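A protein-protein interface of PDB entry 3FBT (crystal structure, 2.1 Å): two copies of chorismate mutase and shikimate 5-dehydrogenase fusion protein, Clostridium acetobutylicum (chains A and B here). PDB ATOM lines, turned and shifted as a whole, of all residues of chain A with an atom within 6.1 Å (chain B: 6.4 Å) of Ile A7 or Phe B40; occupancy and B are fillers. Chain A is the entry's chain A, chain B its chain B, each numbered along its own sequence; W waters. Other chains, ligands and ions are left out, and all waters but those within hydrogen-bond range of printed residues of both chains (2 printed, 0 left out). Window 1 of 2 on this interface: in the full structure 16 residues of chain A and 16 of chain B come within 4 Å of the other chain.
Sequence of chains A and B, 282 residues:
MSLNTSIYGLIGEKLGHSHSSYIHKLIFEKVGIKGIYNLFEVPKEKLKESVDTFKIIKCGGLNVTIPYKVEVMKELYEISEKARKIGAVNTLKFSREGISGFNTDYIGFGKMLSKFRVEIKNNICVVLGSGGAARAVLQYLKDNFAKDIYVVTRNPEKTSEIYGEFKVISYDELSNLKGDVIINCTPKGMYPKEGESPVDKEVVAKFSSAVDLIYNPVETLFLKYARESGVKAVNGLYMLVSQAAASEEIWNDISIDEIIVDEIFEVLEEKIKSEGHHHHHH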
ATOM      1  N   ASN A   4       0.414   5.764 -12.138  1.00  0.00           N
ATOM      2  CA  ASN A   4      -0.699   4.786 -12.176  1.00  0.00           C
ATOM      3  C   ASN A   4      -0.629   3.646 -11.115  1.00  0.00           C
ATOM      4  O   ASN A   4       0.452   3.218 -10.764  1.00  0.00           O
ATOM      5  CB  ASN A   4      -0.772   4.169 -13.573  1.00  0.00           C
ATOM      6  CG  ASN A   4      -1.485   5.047 -14.560  1.00  0.00           C
ATOM      7  OD1 ASN A   4      -1.912   6.155 -14.237  1.00  0.00           O
ATOM      8  ND2 ASN A   4      -1.699   4.532 -15.770  1.00  0.00           N
ATOM      9  N   THR A   5      -1.775   3.161 -10.613  1.00  0.00           N
ATOM     10  CA  THR A   5      -1.755   1.976  -9.746  1.00  0.00           C
ATOM     11  C   THR A   5      -1.865   0.769 -10.686  1.00  0.00           C
ATOM     12  O   THR A   5      -2.668   0.764 -11.564  1.00  0.00           O
ATOM     13  CB  THR A   5      -2.931   1.992  -8.736  1.00  0.00           C
ATOM     14  OG1 THR A   5      -2.794   3.147  -7.922  1.00  0.00           O
ATOM     15  CG2 THR A   5      -2.933   0.750  -7.791  1.00  0.00           C
ATOM     16  N   SER A   6      -0.996  -0.201 -10.570  1.00  0.00           N
ATOM     17  CA  SER A   6      -1.103  -1.411 -11.362  1.00  0.00           C
ATOM     18  C   SER A   6      -2.419  -2.146 -11.060  1.00  0.00           C
ATOM     19  O   SER A   6      -2.735  -2.321  -9.923  1.00  0.00           O
ATOM     20  CB  SER A   6       0.054  -2.322 -11.003  1.00  0.00           C
ATOM     21  OG  SER A   6       1.193  -1.891 -11.709  1.00  0.00           O
ATOM     22  N   ILE A   7      -3.170  -2.535 -12.102  1.00  0.00           N
ATOM     23  CA  ILE A   7      -4.441  -3.217 -11.944  1.00  0.00           C
ATOM     24  C   ILE A   7      -4.261  -4.747 -12.186  1.00  0.00           C
ATOM     25  O   ILE A   7      -3.852  -5.165 -13.252  1.00  0.00           O
ATOM     26  CB  ILE A   7      -5.479  -2.649 -12.957  1.00  0.00           C
ATOM     27  CG1 ILE A   7      -5.679  -1.126 -12.772  1.00  0.00           C
ATOM     28  CG2 ILE A   7      -6.812  -3.436 -12.855  1.00  0.00           C
ATOM     29  CD1 ILE A   7      -6.282  -0.484 -13.961  1.00  0.00           C
ATOM     30  N   TYR A   8      -4.605  -5.587 -11.225  1.00  0.00           N
ATOM     31  CA  TYR A   8      -4.477  -7.052 -11.410  1.00  0.00           C
ATOM     32  C   TYR A   8      -5.888  -7.539 -11.067  1.00  0.00           C
ATOM     33  O   TYR A   8      -6.729  -6.723 -10.636  1.00  0.00           O
ATOM     34  CB  TYR A   8      -3.525  -7.638 -10.378  1.00  0.00           C
ATOM     35  CG  TYR A   8      -2.132  -7.050 -10.356  1.00  0.00           C
ATOM     36  CD1 TYR A   8      -1.085  -7.681 -11.010  1.00  0.00           C
ATOM     37  CD2 TYR A   8      -1.837  -5.907  -9.609  1.00  0.00           C
ATOM     38  CE1 TYR A   8       0.170  -7.211 -10.943  1.00  0.00           C
ATOM     39  CE2 TYR A   8      -0.567  -5.415  -9.561  1.00  0.00           C
ATOM     40  CZ  TYR A   8       0.433  -6.076 -10.249  1.00  0.00           C
ATOM     41  OH  TYR A   8       1.721  -5.632 -10.203  1.00  0.00           O
ATOM     42  N   GLY A   9      -6.181  -8.820 -11.279  1.00  0.00           N
ATOM     43  CA  GLY A   9      -7.520  -9.298 -11.022  1.00  0.00           C
ATOM     44  C   GLY A   9      -7.739 -10.729 -11.400  1.00  0.00           C
ATOM     45  O   GLY A   9      -6.797 -11.437 -11.817  1.00  0.00           O
ATOM     46  N   LYS A  34       2.505  -1.305  -5.467  1.00  0.00           N
ATOM     47  CA  LYS A  34       1.265  -0.474  -5.398  1.00  0.00           C
ATOM     48  C   LYS A  34       0.275  -1.047  -6.426  1.00  0.00           C
ATOM     49  O   LYS A  34       0.495  -0.903  -7.615  1.00  0.00           O
ATOM     50  CB  LYS A  34       1.534   0.989  -5.752  1.00  0.00           C
ATOM     51  CG  LYS A  34       0.403   1.935  -5.234  1.00  0.00           C
ATOM     52  CD  LYS A  34       0.512   3.364  -5.816  1.00  0.00           C
ATOM     53  CE  LYS A  34       1.323   3.364  -7.141  1.00  0.00           C
ATOM     54  NZ  LYS A  34       1.562   4.777  -7.602  1.00  0.00           N
ATOM     55  N   GLY A  35      -0.801  -1.682  -5.973  1.00  0.00           N
ATOM     56  CA  GLY A  35      -1.605  -2.501  -6.841  1.00  0.00           C
ATOM     57  C   GLY A  35      -2.954  -2.737  -6.224  1.00  0.00           C
ATOM     58  O   GLY A  35      -3.155  -2.491  -5.017  1.00  0.00           O
ATOM     59  N   ILE A  36      -3.899  -3.131  -7.068  1.00  0.00           N
ATOM     60  CA  ILE A  36      -5.191  -3.635  -6.595  1.00  0.00           C
ATOM     61  C   ILE A  36      -5.475  -4.947  -7.331  1.00  0.00           C
ATOM     62  O   ILE A  36      -4.954  -5.167  -8.449  1.00  0.00           O
ATOM     63  CB  ILE A  36      -6.341  -2.669  -7.001  1.00  0.00           C
ATOM     64  CG1 ILE A  36      -6.487  -2.646  -8.537  1.00  0.00           C
ATOM     65  CG2 ILE A  36      -6.121  -1.230  -6.374  1.00  0.00           C
ATOM     66  CD1 ILE A  36      -7.709  -1.780  -9.067  1.00  0.00           C
ATOM     67  N   TYR A  37      -6.361  -5.766  -6.770  1.00  0.00           N
ATOM     68  CA  TYR A  37      -6.740  -7.052  -7.368  1.00  0.00           C
ATOM     69  C   TYR A  37      -8.260  -7.099  -7.237  1.00  0.00           C
ATOM     70  O   TYR A  37      -8.773  -7.164  -6.136  1.00  0.00           O
ATOM     71  CB  TYR A  37      -6.116  -8.260  -6.566  1.00  0.00           C
ATOM     72  CG  TYR A  37      -6.299  -9.616  -7.219  1.00  0.00           C
ATOM     73  CD1 TYR A  37      -5.284 -10.162  -8.031  1.00  0.00           C
ATOM     74  CD2 TYR A  37      -7.485 -10.371  -7.033  1.00  0.00           C
ATOM     75  CE1 TYR A  37      -5.442 -11.386  -8.592  1.00  0.00           C
ATOM     76  CE2 TYR A  37      -7.653 -11.623  -7.668  1.00  0.00           C
ATOM     77  CZ  TYR A  37      -6.610 -12.105  -8.401  1.00  0.00           C
ATOM     78  OH  TYR A  37      -6.696 -13.265  -9.077  1.00  0.00           O
ATOM     79  N   ASN A  38      -8.939  -7.070  -8.368  1.00  0.00           N
ATOM     80  CA  ASN A  38     -10.354  -7.046  -8.449  1.00  0.00           C
ATOM     81  C   ASN A  38     -10.875  -8.306  -9.144  1.00  0.00           C
ATOM     82  O   ASN A  38     -10.188  -8.887  -9.981  1.00  0.00           O
ATOM     83  CB  ASN A  38     -10.781  -5.832  -9.318  1.00  0.00           C
ATOM     84  CG  ASN A  38     -10.828  -4.554  -8.526  1.00  0.00           C
ATOM     85  OD1 ASN A  38     -10.402  -4.494  -7.362  1.00  0.00           O
ATOM     86  ND2 ASN A  38     -11.341  -3.533  -9.127  1.00  0.00           N
ATOM     87  N   PHE A  40     -13.329  -9.520 -11.874  1.00  0.00           N
ATOM     88  CA  PHE A  40     -13.930  -8.955 -13.072  1.00  0.00           C
ATOM     89  C   PHE A  40     -14.872  -9.959 -13.695  1.00  0.00           C
ATOM     90  O   PHE A  40     -14.419 -10.988 -14.267  1.00  0.00           O
ATOM     91  CB  PHE A  40     -12.831  -8.611 -14.124  1.00  0.00           C
ATOM     92  CG  PHE A  40     -11.840  -7.563 -13.667  1.00  0.00           C
ATOM     93  CD1 PHE A  40     -12.269  -6.309 -13.340  1.00  0.00           C
ATOM     94  CD2 PHE A  40     -10.471  -7.835 -13.565  1.00  0.00           C
ATOM     95  CE1 PHE A  40     -11.387  -5.318 -12.897  1.00  0.00           C
ATOM     96  CE2 PHE A  40      -9.573  -6.864 -13.112  1.00  0.00           C
ATOM     97  CZ  PHE A  40     -10.040  -5.589 -12.810  1.00  0.00           C
ATOM     98  N   PHE A  54      -7.722  -5.050 -21.676  1.00  0.00           N
ATOM     99  CA  PHE A  54      -6.740  -5.164 -20.589  1.00  0.00           C
ATOM    100  C   PHE A  54      -5.333  -4.955 -21.133  1.00  0.00           C
ATOM    101  O   PHE A  54      -4.452  -4.333 -20.527  1.00  0.00           O
ATOM    102  CB  PHE A  54      -6.852  -6.527 -19.873  1.00  0.00           C
ATOM    103  CG  PHE A  54      -8.018  -6.592 -18.899  1.00  0.00           C
ATOM    104  CD1 PHE A  54      -8.020  -5.803 -17.771  1.00  0.00           C
ATOM    105  CD2 PHE A  54      -9.107  -7.429 -19.134  1.00  0.00           C
ATOM    106  CE1 PHE A  54      -9.112  -5.839 -16.886  1.00  0.00           C
ATOM    107  CE2 PHE A  54     -10.204  -7.448 -18.265  1.00  0.00           C
ATOM    108  CZ  PHE A  54     -10.202  -6.656 -17.131  1.00  0.00           C
ATOM    109  N   ILE A  57      -4.998  -1.050 -21.610  1.00  0.00           N
ATOM    110  CA  ILE A  57      -4.731  -0.268 -20.403  1.00  0.00           C
ATOM    111  C   ILE A  57      -3.551  -0.774 -19.593  1.00  0.00           C
ATOM    112  O   ILE A  57      -3.335  -0.321 -18.510  1.00  0.00           O
ATOM    113  CB  ILE A  57      -5.965  -0.189 -19.544  1.00  0.00           C
ATOM    114  CG1 ILE A  57      -6.269  -1.525 -18.862  1.00  0.00           C
ATOM    115  CG2 ILE A  57      -7.152   0.224 -20.415  1.00  0.00           C
ATOM    116  CD1 ILE A  57      -7.509  -1.438 -18.044  1.00  0.00           C
ATOM    117  N   LYS A  58      -2.753  -1.681 -20.129  1.00  0.00           N
ATOM    118  CA  LYS A  58      -1.541  -2.157 -19.423  1.00  0.00           C
ATOM    119  C   LYS A  58      -1.827  -2.873 -18.108  1.00  0.00           C
ATOM    120  O   LYS A  58      -1.161  -2.631 -17.118  1.00  0.00           O
ATOM    121  CB  LYS A  58      -0.607  -0.973 -19.141  1.00  0.00           C
ATOM    122  CG  LYS A  58      -0.469  -0.095 -20.375  1.00  0.00           C
ATOM    123  CD  LYS A  58       0.765  -0.582 -21.107  1.00  0.00           C
ATOM    124  CE  LYS A  58       1.958   0.031 -20.418  1.00  0.00           C
ATOM    125  NZ  LYS A  58       1.955   1.496 -20.707  1.00  0.00           N
ATOM    126  N   CYS A  59      -2.889  -3.652 -18.075  1.00  0.00           N
ATOM    127  CA  CYS A  59      -3.150  -4.553 -16.932  1.00  0.00           C
ATOM    128  C   CYS A  59      -1.887  -5.149 -16.347  1.00  0.00           C
ATOM    129  O   CYS A  59      -1.043  -5.686 -17.080  1.00  0.00           O
ATOM    130  CB  CYS A  59      -4.026  -5.690 -17.449  1.00  0.00           C
ATOM    131  SG  CYS A  59      -4.508  -6.798 -16.183  1.00  0.00           S
ATOM    132  N   GLY A  60      -1.721  -5.122 -15.039  1.00  0.00           N
ATOM    133  CA  GLY A  60      -0.515  -5.759 -14.453  1.00  0.00           C
ATOM    134  C   GLY A  60      -0.448  -7.313 -14.570  1.00  0.00           C
ATOM    135  O   GLY A  60       0.637  -7.921 -14.417  1.00  0.00           O
ATOM    136  N   GLY A  61      -1.604  -7.954 -14.717  1.00  0.00           N
ATOM    137  CA  GLY A  61      -1.685  -9.429 -14.671  1.00  0.00           C
ATOM    138  C   GLY A  61      -3.054  -9.875 -14.253  1.00  0.00           C
ATOM    139  O   GLY A  61      -3.695  -9.172 -13.498  1.00  0.00           O
ATOM    140  N   LEU A  62      -3.548 -10.966 -14.854  1.00  0.00           N
ATOM    141  CA  LEU A  62      -4.902 -11.555 -14.579  1.00  0.00           C
ATOM    142  C   LEU A  62      -4.851 -13.037 -14.236  1.00  0.00           C
ATOM    143  O   LEU A  62      -4.139 -13.802 -14.872  1.00  0.00           O
ATOM    144  CB  LEU A  62      -5.849 -11.470 -15.813  1.00  0.00           C
ATOM    145  CG  LEU A  62      -6.397 -10.112 -16.269  1.00  0.00           C
ATOM    146  CD1 LEU A  62      -7.407 -10.160 -17.484  1.00  0.00           C
ATOM    147  CD2 LEU A  62      -7.057  -9.480 -15.095  1.00  0.00           C
ATOM    148  N   ILE B   7     -12.348   1.669 -10.058  1.00  0.00           N
ATOM    149  CA  ILE B   7     -11.377   2.156 -10.972  1.00  0.00           C
ATOM    150  C   ILE B   7     -11.922   3.426 -11.699  1.00  0.00           C
ATOM    151  O   ILE B   7     -12.976   3.407 -12.327  1.00  0.00           O
ATOM    152  CB  ILE B   7     -11.057   1.062 -12.011  1.00  0.00           C
ATOM    153  CG1 ILE B   7     -10.483  -0.159 -11.230  1.00  0.00           C
ATOM    154  CG2 ILE B   7     -10.060   1.628 -13.041  1.00  0.00           C
ATOM    155  CD1 ILE B   7     -10.457  -1.460 -12.077  1.00  0.00           C
ATOM    156  N   TYR B   8     -11.207   4.530 -11.532  1.00  0.00           N
ATOM    157  CA  TYR B   8     -11.496   5.746 -12.219  1.00  0.00           C
ATOM    158  C   TYR B   8     -10.268   6.055 -13.062  1.00  0.00           C
ATOM    159  O   TYR B   8      -9.238   5.385 -12.922  1.00  0.00           O
ATOM    160  CB  TYR B   8     -11.660   6.840 -11.189  1.00  0.00           C
ATOM    161  CG  TYR B   8     -12.729   6.590 -10.149  1.00  0.00           C
ATOM    162  CD1 TYR B   8     -14.000   7.092 -10.303  1.00  0.00           C
ATOM    163  CD2 TYR B   8     -12.436   5.874  -8.960  1.00  0.00           C
ATOM    164  CE1 TYR B   8     -14.976   6.917  -9.304  1.00  0.00           C
ATOM    165  CE2 TYR B   8     -13.384   5.662  -7.986  1.00  0.00           C
ATOM    166  CZ  TYR B   8     -14.667   6.186  -8.173  1.00  0.00           C
ATOM    167  OH  TYR B   8     -15.629   6.015  -7.212  1.00  0.00           O
ATOM    168  N   GLY B   9     -10.384   7.031 -13.962  1.00  0.00           N
ATOM    169  CA  GLY B   9      -9.244   7.734 -14.503  1.00  0.00           C
ATOM    170  C   GLY B   9      -9.572   8.596 -15.746  1.00  0.00           C
ATOM    171  O   GLY B   9     -10.725   9.072 -15.931  1.00  0.00           O
ATOM    172  N   LEU B  10      -8.549   8.792 -16.578  1.00  0.00           N
ATOM    173  CA  LEU B  10      -8.620   9.687 -17.740  1.00  0.00           C
ATOM    174  C   LEU B  10      -8.329   8.972 -19.049  1.00  0.00           C
ATOM    175  O   LEU B  10      -7.328   8.327 -19.219  1.00  0.00           O
ATOM    176  CB  LEU B  10      -7.673  10.881 -17.565  1.00  0.00           C
ATOM    177  CG  LEU B  10      -7.422  11.764 -18.812  1.00  0.00           C
ATOM    178  CD1 LEU B  10      -8.691  12.525 -19.144  1.00  0.00           C
ATOM    179  CD2 LEU B  10      -6.269  12.721 -18.481  1.00  0.00           C
ATOM    180  N   ILE B  11      -9.212   9.080 -19.997  1.00  0.00           N
ATOM    181  CA  ILE B  11      -8.916   8.468 -21.278  1.00  0.00           C
ATOM    182  C   ILE B  11      -8.505   9.517 -22.362  1.00  0.00           C
ATOM    183  O   ILE B  11      -9.222  10.495 -22.604  1.00  0.00           O
ATOM    184  CB  ILE B  11     -10.167   7.776 -21.730  1.00  0.00           C
ATOM    185  CG1 ILE B  11      -9.860   6.748 -22.783  1.00  0.00           C
ATOM    186  CG2 ILE B  11     -11.161   8.782 -22.209  1.00  0.00           C
ATOM    187  CD1 ILE B  11     -11.061   5.870 -23.024  1.00  0.00           C
ATOM    188  N   GLY B  12      -7.348   9.330 -22.972  1.00  0.00           N
ATOM    189  CA  GLY B  12      -7.000  10.068 -24.181  1.00  0.00           C
ATOM    190  C   GLY B  12      -5.944   9.279 -24.964  1.00  0.00           C
ATOM    191  O   GLY B  12      -5.472   8.272 -24.504  1.00  0.00           O
ATOM    192  N   GLU B  13      -5.569   9.771 -26.146  1.00  0.00           N
ATOM    193  CA  GLU B  13      -4.578   9.113 -27.021  1.00  0.00           C
ATOM    194  C   GLU B  13      -3.168   9.145 -26.448  1.00  0.00           C
ATOM    195  O   GLU B  13      -2.593   8.106 -26.107  1.00  0.00           O
ATOM    196  CB  GLU B  13      -4.550   9.815 -28.355  1.00  0.00           C
ATOM    197  CG  GLU B  13      -4.219   8.936 -29.536  1.00  0.00           C
ATOM    198  CD  GLU B  13      -4.372   9.714 -30.837  1.00  0.00           C
ATOM    199  OE1 GLU B  13      -4.857   9.135 -31.832  1.00  0.00           O
ATOM    200  OE2 GLU B  13      -4.049  10.926 -30.831  1.00  0.00           O
ATOM    201  N   LEU B  15      -0.845  10.901 -23.452  1.00  0.00           N
ATOM    202  CA  LEU B  15      -0.988  11.614 -22.189  1.00  0.00           C
ATOM    203  C   LEU B  15       0.363  11.875 -21.531  1.00  0.00           C
ATOM    204  O   LEU B  15       1.199  10.962 -21.368  1.00  0.00           O
ATOM    205  CB  LEU B  15      -1.898  10.840 -21.216  1.00  0.00           C
ATOM    206  CG  LEU B  15      -3.343  10.648 -21.695  1.00  0.00           C
ATOM    207  CD1 LEU B  15      -4.107   9.693 -20.851  1.00  0.00           C
ATOM    208  CD2 LEU B  15      -4.037  11.968 -21.721  1.00  0.00           C
ATOM    209  N   ILE B  36      -8.898   4.213  -7.307  1.00  0.00           N
ATOM    210  CA  ILE B  36      -7.663   4.702  -7.830  1.00  0.00           C
ATOM    211  C   ILE B  36      -8.056   5.463  -9.061  1.00  0.00           C
ATOM    212  O   ILE B  36      -9.120   5.170  -9.634  1.00  0.00           O
ATOM    213  CB  ILE B  36      -6.774   3.504  -8.314  1.00  0.00           C
ATOM    214  CG1 ILE B  36      -7.545   2.694  -9.314  1.00  0.00           C
ATOM    215  CG2 ILE B  36      -6.386   2.642  -7.110  1.00  0.00           C
ATOM    216  CD1 ILE B  36      -6.663   1.558 -10.063  1.00  0.00           C
ATOM    217  N   TYR B  37      -7.174   6.349  -9.522  1.00  0.00           N
ATOM    218  CA  TYR B  37      -7.490   7.109 -10.745  1.00  0.00           C
ATOM    219  C   TYR B  37      -6.257   6.887 -11.648  1.00  0.00           C
ATOM    220  O   TYR B  37      -5.164   7.330 -11.269  1.00  0.00           O
ATOM    221  CB  TYR B  37      -7.578   8.617 -10.393  1.00  0.00           C
ATOM    222  CG  TYR B  37      -7.988   9.513 -11.511  1.00  0.00           C
ATOM    223  CD1 TYR B  37      -9.320   9.857 -11.696  1.00  0.00           C
ATOM    224  CD2 TYR B  37      -7.048  10.044 -12.398  1.00  0.00           C
ATOM    225  CE1 TYR B  37      -9.699  10.678 -12.742  1.00  0.00           C
ATOM    226  CE2 TYR B  37      -7.460  10.853 -13.418  1.00  0.00           C
ATOM    227  CZ  TYR B  37      -8.758  11.159 -13.576  1.00  0.00           C
ATOM    228  OH  TYR B  37      -9.147  11.976 -14.618  1.00  0.00           O
ATOM    229  N   ASN B  38      -6.405   6.213 -12.782  1.00  0.00           N
ATOM    230  CA  ASN B  38      -5.212   6.020 -13.653  1.00  0.00           C
ATOM    231  C   ASN B  38      -5.315   6.856 -14.938  1.00  0.00           C
ATOM    232  O   ASN B  38      -6.396   7.161 -15.369  1.00  0.00           O
ATOM    233  CB  ASN B  38      -5.046   4.545 -14.116  1.00  0.00           C
ATOM    234  CG  ASN B  38      -4.419   3.633 -13.032  1.00  0.00           C
ATOM    235  OD1 ASN B  38      -4.085   4.083 -11.935  1.00  0.00           O
ATOM    236  ND2 ASN B  38      -4.192   2.365 -13.385  1.00  0.00           N
ATOM    237  N   LEU B  39      -4.168   7.160 -15.551  1.00  0.00           N
ATOM    238  CA  LEU B  39      -4.137   7.638 -16.920  1.00  0.00           C
ATOM    239  C   LEU B  39      -4.218   6.484 -17.957  1.00  0.00           C
ATOM    240  O   LEU B  39      -3.381   5.626 -18.028  1.00  0.00           O
ATOM    241  CB  LEU B  39      -2.857   8.475 -17.159  1.00  0.00           C
ATOM    242  CG  LEU B  39      -2.533   9.668 -16.251  1.00  0.00           C
ATOM    243  CD1 LEU B  39      -1.550  10.605 -17.008  1.00  0.00           C
ATOM    244  CD2 LEU B  39      -3.809  10.398 -15.865  1.00  0.00           C
ATOM    245  N   PHE B  40      -5.231   6.464 -18.769  1.00  0.00           N
ATOM    246  CA  PHE B  40      -5.360   5.361 -19.686  1.00  0.00           C
ATOM    247  C   PHE B  40      -5.129   5.821 -21.161  1.00  0.00           C
ATOM    248  O   PHE B  40      -5.893   6.664 -21.738  1.00  0.00           O
ATOM    249  CB  PHE B  40      -6.743   4.746 -19.538  1.00  0.00           C
ATOM    250  CG  PHE B  40      -7.051   4.131 -18.159  1.00  0.00           C
ATOM    251  CD1 PHE B  40      -6.371   3.014 -17.701  1.00  0.00           C
ATOM    252  CD2 PHE B  40      -8.104   4.603 -17.412  1.00  0.00           C
ATOM    253  CE1 PHE B  40      -6.726   2.380 -16.461  1.00  0.00           C
ATOM    254  CE2 PHE B  40      -8.481   3.980 -16.210  1.00  0.00           C
ATOM    255  CZ  PHE B  40      -7.736   2.850 -15.739  1.00  0.00           C
ATOM    256  N   GLU B  41      -4.068   5.290 -21.778  1.00  0.00           N
ATOM    257  CA  GLU B  41      -3.768   5.653 -23.165  1.00  0.00           C
ATOM    258  C   GLU B  41      -4.534   4.728 -24.122  1.00  0.00           C
ATOM    259  O   GLU B  41      -4.313   3.518 -24.177  1.00  0.00           O
ATOM    260  CB  GLU B  41      -2.240   5.723 -23.421  1.00  0.00           C
ATOM    261  CG  GLU B  41      -1.574   6.890 -22.618  1.00  0.00           C
ATOM    262  CD  GLU B  41      -0.136   7.287 -23.088  1.00  0.00           C
ATOM    263  OE1 GLU B  41       0.818   6.493 -22.888  1.00  0.00           O
ATOM    264  OE2 GLU B  41       0.060   8.424 -23.605  1.00  0.00           O
ATOM    265  N   VAL B  42      -5.473   5.289 -24.855  1.00  0.00           N
ATOM    266  CA  VAL B  42      -6.270   4.529 -25.800  1.00  0.00           C
ATOM    267  C   VAL B  42      -6.015   5.085 -27.216  1.00  0.00           C
ATOM    268  O   VAL B  42      -6.066   6.320 -27.434  1.00  0.00           O
ATOM    269  CB  VAL B  42      -7.793   4.636 -25.449  1.00  0.00           C
ATOM    270  CG1 VAL B  42      -8.675   3.865 -26.427  1.00  0.00           C
ATOM    271  CG2 VAL B  42      -8.040   4.159 -23.999  1.00  0.00           C
ATOM    272  N   PHE B  54     -14.835  -0.895 -20.195  1.00  0.00           N
ATOM    273  CA  PHE B  54     -14.990  -0.233 -18.914  1.00  0.00           C
ATOM    274  C   PHE B  54     -16.404  -0.453 -18.374  1.00  0.00           C
ATOM    275  O   PHE B  54     -16.592  -0.778 -17.215  1.00  0.00           O
ATOM    276  CB  PHE B  54     -14.584   1.232 -18.980  1.00  0.00           C
ATOM    277  CG  PHE B  54     -13.110   1.432 -18.839  1.00  0.00           C
ATOM    278  CD1 PHE B  54     -12.503   1.374 -17.598  1.00  0.00           C
ATOM    279  CD2 PHE B  54     -12.318   1.648 -19.930  1.00  0.00           C
ATOM    280  CE1 PHE B  54     -11.162   1.573 -17.483  1.00  0.00           C
ATOM    281  CE2 PHE B  54     -10.949   1.868 -19.776  1.00  0.00           C
ATOM    282  CZ  PHE B  54     -10.391   1.812 -18.588  1.00  0.00           C
ATOM    283  N   CYS B  59     -16.549   0.295 -14.330  1.00  0.00           N
ATOM    284  CA  CYS B  59     -15.637   1.408 -14.093  1.00  0.00           C
ATOM    285  C   CYS B  59     -16.329   2.445 -13.236  1.00  0.00           C
ATOM    286  O   CYS B  59     -17.499   2.716 -13.439  1.00  0.00           O
ATOM    287  CB  CYS B  59     -15.391   2.059 -15.460  1.00  0.00           C
ATOM    288  SG  CYS B  59     -14.374   3.510 -15.319  1.00  0.00           S
ATOM    289  N   LEU B  62     -15.026   7.936 -15.828  1.00  0.00           N
ATOM    290  CA  LEU B  62     -13.883   8.370 -16.646  1.00  0.00           C
ATOM    291  C   LEU B  62     -13.975   9.860 -17.048  1.00  0.00           C
ATOM    292  O   LEU B  62     -15.011  10.345 -17.440  1.00  0.00           O
ATOM    293  CB  LEU B  62     -13.814   7.520 -17.927  1.00  0.00           C
ATOM    294  CG  LEU B  62     -13.389   6.060 -17.840  1.00  0.00           C
ATOM    295  CD1 LEU B  62     -13.529   5.414 -19.229  1.00  0.00           C
ATOM    296  CD2 LEU B  62     -11.921   5.952 -17.392  1.00  0.00           C
HETATM  297  O   HOH W   1      -3.609   5.478  -9.104  1.00  0.00           O
HETATM  298  O   HOH W   2      -3.442   1.072 -15.723  1.00  0.00           O
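Ile A7 touches Ile B36, and with the chains exchanged Ile A36 touches Ile B7.
Ile A7 touches Asn B38, and with the chains exchanged Asn A38 touches Ile B7.
Ile A7 touches Phe B40, but with the chains exchanged Phe A40 does not touch Ile B7 (4.1 Å).
Ile B36 touches its own counterpart, Ile A36.
Positions printed for both chains: 7, 8, 9, 36, 37, 38, 40, 54, 59 and 62.
Of the 11 pairs that touch across the chains among the printed residues, 5 have their exchanged pair printed and touching as well.
Of the 19 printed residues of chain A, 6 touch a printed residue of chain B.
Printed residues of chain A that touch a printed residue of chain B: Asn A4, Thr A5, Ile A7, Ile A36, Asn A38 and Ile A57.
Hydrophobic or aromatic side chains of chain A within 4 Å of the printed part of chain B: Ile A7, Ile A36 and Ile A57.
Of the 18 printed residues of chain B, 5 touch a printed residue of chain A.
Along chain B the printed residues that touch a printed residue of chain A span positions 7 to 40.
Among the printed residues, 11 pairs touch across the chains.
Among the printed residues, no Asp or Glu carboxylate lies within 4 Å of a Lys or Arg side-chain nitrogen of the other chain.
The backbone carbonyl oxygen (O) of Ile B7 lies within hydrogen-bond range of the side-chain sulfur (SG) of Cys B59 (3.3 Å).
N of Ile A36 is in hydrogen-bond range of O of Ser A6.
The backbone NH of Tyr A8 lies within hydrogen-bond range of the backbone carbonyl oxygen of Ile A36, 2.8 Å away.
N of Tyr B8 is in hydrogen-bond range of O of Ile B36 (2.9 Å).
The backbone carbonyl oxygen of Tyr A8 lies within hydrogen-bond range of the backbone NH of Asn A38, 3.2 Å away.
The side-chain sulfur (SG) of Cys A59 lies within hydrogen-bond range of the backbone carbonyl oxygen (O) of Ile A7 (3.4 Å).
Ile A7 touches just these residues of chain B: Ile B36, Asn B38 and Phe B40.
Of the printed residues of chain B, Ile A57 touches Phe B40 (3.7 Å).
Of the printed residues of chain A, Leu B39 touches Asn A4 (2.8 Å).
The nearest residue of chain B that does not touch Ile A7 is Ile B7 (4.2 Å).
Asn A4 touches Asn B38.
Thr A5 touches Ile B36.
CG1 of Ile A7 touches CD1 of Ile B36 (3.9 Å).
CD1 of Ile A7 touches ND2 of Asn B38, at 3.6 Å.
CD1 of Ile A7 touches CE1 of Phe B40, 3.8 Å away.
CD1 of Ile A36 touches CG1 of Ile B7 (3.9 Å).
CD1 of Ile A36 touches CD1 of Ile B36, at 3.6 Å.
ND2 of Asn A38 touches CD1 of Ile B7, 3.7 Å away.
Ile A57 touches Phe B40 (CB to CD1, 3.7 Å).
Water W1 lies within hydrogen-bond range of OG1 of Thr A5, OD1 of Asn B38 and O of Tyr B37.
Water W2 bridges the side-chain amide nitrogen of Asn B38 and the backbone carbonyl oxygen of Ile A57.
The backbone NH (N) of Thr A5 lies within hydrogen-bond range of the side-chain amide oxygen (OD1) of Asn B38, 2.8 Å away.
N of Leu B39 sits at hydrogen-bond distance from OD1 of Asn A4, at 2.8 Å.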
